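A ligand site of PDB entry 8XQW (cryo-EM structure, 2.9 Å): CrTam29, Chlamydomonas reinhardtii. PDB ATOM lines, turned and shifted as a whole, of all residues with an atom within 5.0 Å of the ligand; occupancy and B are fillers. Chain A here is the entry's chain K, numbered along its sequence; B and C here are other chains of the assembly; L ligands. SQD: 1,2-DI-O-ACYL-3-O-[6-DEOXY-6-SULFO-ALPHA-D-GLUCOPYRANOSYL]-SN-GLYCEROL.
NE1 of Trp 145 sits at hydrogen-bond distance from O9 of the ligand. An oxygen (O4) of the ligand sits at hydrogen-bond distance from the backbone carbonyl oxygen (O) of Glu 135 (2.7 Å).
OXT of Phe 255 lies within salt-bridge range of NH2 of Arg 137 (3.5 Å). The side-chain carboxylate (OE1) of Glu 135 is in salt-bridge range of the guanidinium group (NE) of Arg 212 of chain B. N of Leu 140 sits at hydrogen-bond distance from O of Leu 254. The side-chain carboxylate (OE2) of Glu 135 is in salt-bridge range of the guanidinium group (NH1) of Arg 248, 3.5 Å away. The side-chain amide oxygen of Gln 149 lies within hydrogen-bond range of the indole nitrogen of Trp 145, at 2.8 Å. The backbone NH (N) of Phe 141 sits at hydrogen-bond distance from the backbone carbonyl oxygen (O) of Leu 254, at 3.0 Å.
Arg 137 touches the ligand. Phe 141 touches the ligand. NH2 of Arg 248 touches C46 of the ligand (3.8 Å). Leu 254 touches the ligand. Phe 255 touches the ligand (CD2 to C30, 3.5 Å). Trp 209 of chain B touches the ligand (CD1 to O8, 3.5 Å). Hydrophobic or aromatic side chains within 4 Å of the ligand: Phe 141, Trp 145, Leu 254, Phe 255 and Trp 209 of chain B. Within 4 Å of the ligand: Glu 135, Arg 137, Phe 141, Trp 145, Arg 248, Leu 254, Phe 255 and Trp 209 of chain B. The nearest printed residue that does not touch the ligand is Gln 149 (4.01 Å).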
ATOM      1  N   ALA A 134     -12.587   1.792   4.109  1.00  0.00           N
ATOM      2  CA  ALA A 134     -12.569   0.889   5.244  1.00  0.00           C
ATOM      3  C   ALA A 134     -11.825   1.477   6.415  1.00  0.00           C
ATOM      4  O   ALA A 134     -11.967   0.992   7.537  1.00  0.00           O
ATOM      5  CB  ALA A 134     -11.951  -0.447   4.853  1.00  0.00           C
ATOM      6  N   GLU A 135     -11.036   2.519   6.177  1.00  0.00           N
ATOM      7  CA  GLU A 135     -10.451   3.337   7.212  1.00  0.00           C
ATOM      8  C   GLU A 135     -11.346   4.489   7.592  1.00  0.00           C
ATOM      9  O   GLU A 135     -10.960   5.334   8.404  1.00  0.00           O
ATOM     10  CB  GLU A 135      -9.098   3.856   6.748  1.00  0.00           C
ATOM     11  CG  GLU A 135      -8.183   2.771   6.280  1.00  0.00           C
ATOM     12  CD  GLU A 135      -6.747   3.202   6.299  1.00  0.00           C
ATOM     13  OE1 GLU A 135      -6.498   4.419   6.302  1.00  0.00           O
ATOM     14  OE2 GLU A 135      -5.851   2.338   6.309  1.00  0.00           O
ATOM     15  N   LYS A 136     -12.546   4.557   7.022  1.00  0.00           N
ATOM     16  CA  LYS A 136     -13.523   5.567   7.389  1.00  0.00           C
ATOM     17  C   LYS A 136     -14.809   4.968   7.934  1.00  0.00           C
ATOM     18  O   LYS A 136     -15.847   5.631   7.891  1.00  0.00           O
ATOM     19  CB  LYS A 136     -13.849   6.444   6.188  1.00  0.00           C
ATOM     20  CG  LYS A 136     -12.659   7.088   5.566  1.00  0.00           C
ATOM     21  CD  LYS A 136     -13.038   7.711   4.276  1.00  0.00           C
ATOM     22  CE  LYS A 136     -12.340   9.003   4.090  1.00  0.00           C
ATOM     23  NZ  LYS A 136     -12.937   9.743   2.964  1.00  0.00           N
ATOM     24  N   ARG A 137     -14.777   3.741   8.431  1.00  0.00           N
ATOM     25  CA  ARG A 137     -15.952   3.163   9.039  1.00  0.00           C
ATOM     26  C   ARG A 137     -16.115   3.700  10.443  1.00  0.00           C
ATOM     27  O   ARG A 137     -15.167   3.743  11.209  1.00  0.00           O
ATOM     28  CB  ARG A 137     -15.832   1.655   9.080  1.00  0.00           C
ATOM     29  CG  ARG A 137     -16.068   0.977   7.793  1.00  0.00           C
ATOM     30  CD  ARG A 137     -15.786  -0.479   7.942  1.00  0.00           C
ATOM     31  NE  ARG A 137     -16.863  -1.156   8.649  1.00  0.00           N
ATOM     32  CZ  ARG A 137     -16.701  -1.795   9.799  1.00  0.00           C
ATOM     33  NH1 ARG A 137     -17.719  -2.373  10.374  1.00  0.00           N
ATOM     34  NH2 ARG A 137     -15.507  -1.835  10.362  1.00  0.00           N
ATOM     35  N   LEU A 140     -17.961   1.315  17.110  1.00  0.00           N
ATOM     36  CA  LEU A 140     -17.842   1.645  18.524  1.00  0.00           C
ATOM     37  C   LEU A 140     -16.405   1.595  19.006  1.00  0.00           C
ATOM     38  O   LEU A 140     -16.067   2.267  19.982  1.00  0.00           O
ATOM     39  CB  LEU A 140     -18.689   0.718  19.366  1.00  0.00           C
ATOM     40  CG  LEU A 140     -20.202   0.835  19.216  1.00  0.00           C
ATOM     41  CD1 LEU A 140     -20.868  -0.382  19.771  1.00  0.00           C
ATOM     42  CD2 LEU A 140     -20.690   2.043  19.947  1.00  0.00           C
ATOM     43  N   PHE A 141     -15.541   0.806  18.376  1.00  0.00           N
ATOM     44  CA  PHE A 141     -14.151   0.812  18.788  1.00  0.00           C
ATOM     45  C   PHE A 141     -13.477   2.112  18.381  1.00  0.00           C
ATOM     46  O   PHE A 141     -12.617   2.609  19.101  1.00  0.00           O
ATOM     47  CB  PHE A 141     -13.411  -0.365  18.179  1.00  0.00           C
ATOM     48  CG  PHE A 141     -11.913  -0.233  18.256  1.00  0.00           C
ATOM     49  CD1 PHE A 141     -11.248  -0.514  19.421  1.00  0.00           C
ATOM     50  CD2 PHE A 141     -11.183   0.179  17.166  1.00  0.00           C
ATOM     51  CE1 PHE A 141      -9.877  -0.383  19.498  1.00  0.00           C
ATOM     52  CE2 PHE A 141      -9.824   0.312  17.250  1.00  0.00           C
ATOM     53  CZ  PHE A 141      -9.175   0.018  18.406  1.00  0.00           C
ATOM     54  N   SER A 142     -13.838   2.654  17.231  1.00  0.00           N
ATOM     55  CA  SER A 142     -13.149   3.831  16.730  1.00  0.00           C
ATOM     56  C   SER A 142     -13.540   5.106  17.443  1.00  0.00           C
ATOM     57  O   SER A 142     -12.733   6.027  17.499  1.00  0.00           O
ATOM     58  CB  SER A 142     -13.422   3.993  15.244  1.00  0.00           C
ATOM     59  OG  SER A 142     -14.659   4.608  15.060  1.00  0.00           O
ATOM     60  N   VAL A 144     -13.638   5.451  20.515  1.00  0.00           N
ATOM     61  CA  VAL A 144     -12.814   5.491  21.711  1.00  0.00           C
ATOM     62  C   VAL A 144     -11.336   5.662  21.370  1.00  0.00           C
ATOM     63  O   VAL A 144     -10.609   6.410  22.030  1.00  0.00           O
ATOM     64  CB  VAL A 144     -13.035   4.200  22.518  1.00  0.00           C
ATOM     65  CG1 VAL A 144     -12.202   4.211  23.754  1.00  0.00           C
ATOM     66  CG2 VAL A 144     -14.480   4.055  22.875  1.00  0.00           C
ATOM     67  N   TRP A 145     -10.891   4.968  20.329  1.00  0.00           N
ATOM     68  CA  TRP A 145      -9.581   5.281  19.789  1.00  0.00           C
ATOM     69  C   TRP A 145      -9.474   6.746  19.418  1.00  0.00           C
ATOM     70  O   TRP A 145      -8.385   7.318  19.467  1.00  0.00           O
ATOM     71  CB  TRP A 145      -9.289   4.398  18.595  1.00  0.00           C
ATOM     72  CG  TRP A 145      -7.891   4.456  18.248  1.00  0.00           C
ATOM     73  CD1 TRP A 145      -7.333   5.118  17.214  1.00  0.00           C
ATOM     74  CD2 TRP A 145      -6.824   3.867  18.971  1.00  0.00           C
ATOM     75  NE1 TRP A 145      -5.990   4.970  17.237  1.00  0.00           N
ATOM     76  CE2 TRP A 145      -5.646   4.207  18.316  1.00  0.00           C
ATOM     77  CE3 TRP A 145      -6.756   3.088  20.115  1.00  0.00           C
ATOM     78  CZ2 TRP A 145      -4.414   3.783  18.751  1.00  0.00           C
ATOM     79  CZ3 TRP A 145      -5.542   2.672  20.546  1.00  0.00           C
ATOM     80  CH2 TRP A 145      -4.378   3.024  19.878  1.00  0.00           C
ATOM     81  N   GLN A 149      -6.233   9.059  20.554  1.00  0.00           N
ATOM     82  CA  GLN A 149      -5.452   9.827  19.595  1.00  0.00           C
ATOM     83  C   GLN A 149      -5.574  11.321  19.830  1.00  0.00           C
ATOM     84  O   GLN A 149      -4.600  12.051  19.635  1.00  0.00           O
ATOM     85  CB  GLN A 149      -5.890   9.484  18.189  1.00  0.00           C
ATOM     86  CG  GLN A 149      -4.758   9.361  17.245  1.00  0.00           C
ATOM     87  CD  GLN A 149      -4.073   8.049  17.363  1.00  0.00           C
ATOM     88  OE1 GLN A 149      -4.515   7.188  18.096  1.00  0.00           O
ATOM     89  NE2 GLN A 149      -2.995   7.874  16.638  1.00  0.00           N
ATOM     90  N   ARG A 248      -7.615  -5.713   7.134  1.00  0.00           N
ATOM     91  CA  ARG A 248      -8.130  -5.064   8.325  1.00  0.00           C
ATOM     92  C   ARG A 248      -9.319  -5.831   8.869  1.00  0.00           C
ATOM     93  O   ARG A 248     -10.263  -6.100   8.124  1.00  0.00           O
ATOM     94  CB  ARG A 248      -8.548  -3.650   7.972  1.00  0.00           C
ATOM     95  CG  ARG A 248      -8.664  -2.730   9.136  1.00  0.00           C
ATOM     96  CD  ARG A 248      -8.952  -1.342   8.661  1.00  0.00           C
ATOM     97  NE  ARG A 248      -8.332  -0.355   9.526  1.00  0.00           N
ATOM     98  CZ  ARG A 248      -7.072   0.045   9.393  1.00  0.00           C
ATOM     99  NH1 ARG A 248      -6.324  -0.452   8.429  1.00  0.00           N
ATOM    100  NH2 ARG A 248      -6.570   0.940  10.211  1.00  0.00           N
ATOM    101  N   PRO A 249      -9.335  -6.198  10.153  1.00  0.00           N
ATOM    102  CA  PRO A 249     -10.461  -6.963  10.676  1.00  0.00           C
ATOM    103  C   PRO A 249     -11.631  -6.052  11.013  1.00  0.00           C
ATOM    104  O   PRO A 249     -11.464  -4.993  11.612  1.00  0.00           O
ATOM    105  CB  PRO A 249      -9.897  -7.620  11.936  1.00  0.00           C
ATOM    106  CG  PRO A 249      -8.564  -7.038  12.144  1.00  0.00           C
ATOM    107  CD  PRO A 249      -8.344  -5.925  11.194  1.00  0.00           C
ATOM    108  N   LEU A 254     -19.592  -2.973  15.980  1.00  0.00           N
ATOM    109  CA  LEU A 254     -18.753  -3.137  17.151  1.00  0.00           C
ATOM    110  C   LEU A 254     -17.333  -2.661  16.894  1.00  0.00           C
ATOM    111  O   LEU A 254     -16.853  -1.732  17.540  1.00  0.00           O
ATOM    112  CB  LEU A 254     -18.747  -4.589  17.605  1.00  0.00           C
ATOM    113  CG  LEU A 254     -17.780  -4.848  18.757  1.00  0.00           C
ATOM    114  CD1 LEU A 254     -18.209  -4.047  19.964  1.00  0.00           C
ATOM    115  CD2 LEU A 254     -17.725  -6.298  19.109  1.00  0.00           C
ATOM    116  N   PHE A 255     -16.616  -3.303  15.987  1.00  0.00           N
ATOM    117  CA  PHE A 255     -15.312  -2.793  15.613  1.00  0.00           C
ATOM    118  C   PHE A 255     -15.015  -3.011  14.145  1.00  0.00           C
ATOM    119  O   PHE A 255     -13.931  -2.720  13.686  1.00  0.00           O
ATOM    120  CB  PHE A 255     -14.196  -3.406  16.476  1.00  0.00           C
ATOM    121  CG  PHE A 255     -13.858  -4.835  16.144  1.00  0.00           C
ATOM    122  CD1 PHE A 255     -12.948  -5.136  15.165  1.00  0.00           C
ATOM    123  CD2 PHE A 255     -14.400  -5.869  16.873  1.00  0.00           C
ATOM    124  CE1 PHE A 255     -12.633  -6.427  14.896  1.00  0.00           C
ATOM    125  CE2 PHE A 255     -14.082  -7.158  16.594  1.00  0.00           C
ATOM    126  CZ  PHE A 255     -13.203  -7.432  15.611  1.00  0.00           C
ATOM    127  OXT PHE A 255     -15.866  -3.465  13.384  1.00  0.00           O
ATOM    128  N   TRP B 209      -4.656  11.803  10.200  1.00  0.00           N
ATOM    129  CA  TRP B 209      -5.632  11.383  11.195  1.00  0.00           C
ATOM    130  C   TRP B 209      -6.919  12.185  11.096  1.00  0.00           C
ATOM    131  O   TRP B 209      -7.993  11.647  11.360  1.00  0.00           O
ATOM    132  CB  TRP B 209      -5.037  11.519  12.602  1.00  0.00           C
ATOM    133  CG  TRP B 209      -6.029  11.507  13.727  1.00  0.00           C
ATOM    134  CD1 TRP B 209      -6.766  10.447  14.150  1.00  0.00           C
ATOM    135  CD2 TRP B 209      -6.365  12.595  14.582  1.00  0.00           C
ATOM    136  NE1 TRP B 209      -7.545  10.820  15.218  1.00  0.00           N
ATOM    137  CE2 TRP B 209      -7.310  12.133  15.494  1.00  0.00           C
ATOM    138  CE3 TRP B 209      -5.943  13.916  14.663  1.00  0.00           C
ATOM    139  CZ2 TRP B 209      -7.852  12.940  16.460  1.00  0.00           C
ATOM    140  CZ3 TRP B 209      -6.490  14.715  15.627  1.00  0.00           C
ATOM    141  CH2 TRP B 209      -7.422  14.221  16.515  1.00  0.00           C
ATOM    142  N   ARG B 212      -9.441  10.845   8.484  1.00  0.00           N
ATOM    143  CA  ARG B 212     -10.026   9.538   8.736  1.00  0.00           C
ATOM    144  C   ARG B 212     -10.983   9.526   9.916  1.00  0.00           C
ATOM    145  O   ARG B 212     -11.507   8.461  10.248  1.00  0.00           O
ATOM    146  CB  ARG B 212      -8.943   8.504   9.001  1.00  0.00           C
ATOM    147  CG  ARG B 212      -8.179   8.068   7.806  1.00  0.00           C
ATOM    148  CD  ARG B 212      -6.899   7.414   8.212  1.00  0.00           C
ATOM    149  NE  ARG B 212      -6.154   6.899   7.071  1.00  0.00           N
ATOM    150  CZ  ARG B 212      -5.460   7.642   6.228  1.00  0.00           C
ATOM    151  NH1 ARG B 212      -5.410   8.947   6.397  1.00  0.00           N
ATOM    152  NH2 ARG B 212      -4.819   7.093   5.217  1.00  0.00           N
ATOM    153  N   SER B 213     -11.219  10.652  10.566  1.00  0.00           N
ATOM    154  CA  SER B 213     -11.940  10.668  11.830  1.00  0.00           C
ATOM    155  C   SER B 213     -12.966  11.768  11.866  1.00  0.00           C
ATOM    156  O   SER B 213     -13.027  12.543  12.815  1.00  0.00           O
ATOM    157  CB  SER B 213     -10.982  10.821  12.996  1.00  0.00           C
ATOM    158  OG  SER B 213     -10.353   9.582  13.271  1.00  0.00           O
ATOM    159  N   MET C 322      -8.616 -13.149  13.572  1.00  0.00           N
ATOM    160  CA  MET C 322      -8.289 -11.772  13.247  1.00  0.00           C
ATOM    161  C   MET C 322      -7.060 -11.660  12.361  1.00  0.00           C
ATOM    162  O   MET C 322      -6.991 -10.763  11.532  1.00  0.00           O
ATOM    163  CB  MET C 322      -8.093 -10.957  14.516  1.00  0.00           C
ATOM    164  CG  MET C 322      -9.355 -10.850  15.338  1.00  0.00           C
ATOM    165  SD  MET C 322      -9.565  -9.250  16.144  1.00  0.00           S
ATOM    166  CE  MET C 322      -8.047  -9.167  17.065  1.00  0.00           C
HETATM  167  O6  SQD L   1      -7.857   2.155  14.755  1.00  0.00           O
HETATM  168  C44 SQD L   1      -6.466   2.116  14.965  1.00  0.00           C
HETATM  169  C45 SQD L   1      -6.011   0.689  15.177  1.00  0.00           C
HETATM  170  C46 SQD L   1      -6.130  -0.064  13.861  1.00  0.00           C
HETATM  171  O47 SQD L   1      -4.691   0.628  15.639  1.00  0.00           O
HETATM  172  C7  SQD L   1      -4.400   0.331  16.997  1.00  0.00           C
HETATM  173  O49 SQD L   1      -3.255   0.414  17.396  1.00  0.00           O
HETATM  174  C8  SQD L   1      -5.400  -0.449  17.838  1.00  0.00           C
HETATM  175  C9  SQD L   1      -4.654  -1.114  18.985  1.00  0.00           C
HETATM  176  C10 SQD L   1      -5.558  -1.206  20.199  1.00  0.00           C
HETATM  177  C11 SQD L   1      -5.820  -2.681  20.526  1.00  0.00           C
HETATM  178  C12 SQD L   1      -6.224  -2.856  21.977  1.00  0.00           C
HETATM  179  C13 SQD L   1      -7.629  -3.455  22.042  1.00  0.00           C
HETATM  180  C14 SQD L   1      -8.153  -3.408  23.465  1.00  0.00           C
HETATM  181  C15 SQD L   1      -8.849  -4.718  23.798  1.00  0.00           C
HETATM  182  O48 SQD L   1      -7.306  -0.847  13.870  1.00  0.00           O
HETATM  183  C23 SQD L   1      -7.227  -2.162  14.365  1.00  0.00           C
HETATM  184  O10 SQD L   1      -6.185  -2.538  14.832  1.00  0.00           O
HETATM  185  C24 SQD L   1      -8.498  -2.888  14.761  1.00  0.00           C
HETATM  186  C25 SQD L   1      -8.255  -3.578  16.089  1.00  0.00           C
HETATM  187  C26 SQD L   1      -9.259  -4.723  16.234  1.00  0.00           C
HETATM  188  C27 SQD L   1     -10.236  -4.398  17.356  1.00  0.00           C
HETATM  189  C28 SQD L   1      -9.672  -4.887  18.692  1.00  0.00           C
HETATM  190  C29 SQD L   1     -10.586  -5.971  19.276  1.00  0.00           C
HETATM  191  C30 SQD L   1     -12.000  -5.410  19.441  1.00  0.00           C
HETATM  192  C31 SQD L   1     -12.040  -4.409  20.603  1.00  0.00           C
HETATM  193  C32 SQD L   1     -13.441  -4.392  21.232  1.00  0.00           C
HETATM  194  C33 SQD L   1     -14.213  -3.173  20.733  1.00  0.00           C
HETATM  195  C34 SQD L   1     -15.150  -2.633  21.815  1.00  0.00           C
HETATM  196  C35 SQD L   1     -14.555  -1.386  22.423  1.00  0.00           C
HETATM  197  C36 SQD L   1     -15.553  -0.777  23.379  1.00  0.00           C
HETATM  198  C1  SQD L   1      -8.291   2.793  13.588  1.00  0.00           C
HETATM  199  C2  SQD L   1      -9.755   2.856  13.401  1.00  0.00           C
HETATM  200  O2  SQD L   1     -10.322   1.646  13.646  1.00  0.00           O
HETATM  201  C3  SQD L   1      -9.901   3.152  11.962  1.00  0.00           C
HETATM  202  O3  SQD L   1     -11.228   3.193  11.634  1.00  0.00           O
HETATM  203  C4  SQD L   1      -9.258   4.440  11.564  1.00  0.00           C
HETATM  204  O4  SQD L   1      -9.093   4.444  10.214  1.00  0.00           O
HETATM  205  C5  SQD L   1      -7.919   4.638  12.180  1.00  0.00           C
HETATM  206  C6  SQD L   1      -7.671   6.114  12.266  1.00  0.00           C
HETATM  207  O5  SQD L   1      -7.759   4.073  13.452  1.00  0.00           O
HETATM  208  S   SQD L   1      -6.050   6.362  12.912  1.00  0.00           S
HETATM  209  O7  SQD L   1      -5.209   5.242  12.638  1.00  0.00           O
HETATM  210  O8  SQD L   1      -5.492   7.624  12.426  1.00  0.00           O
HETATM  211  O9  SQD L   1      -6.037   6.312  14.333  1.00  0.00           O
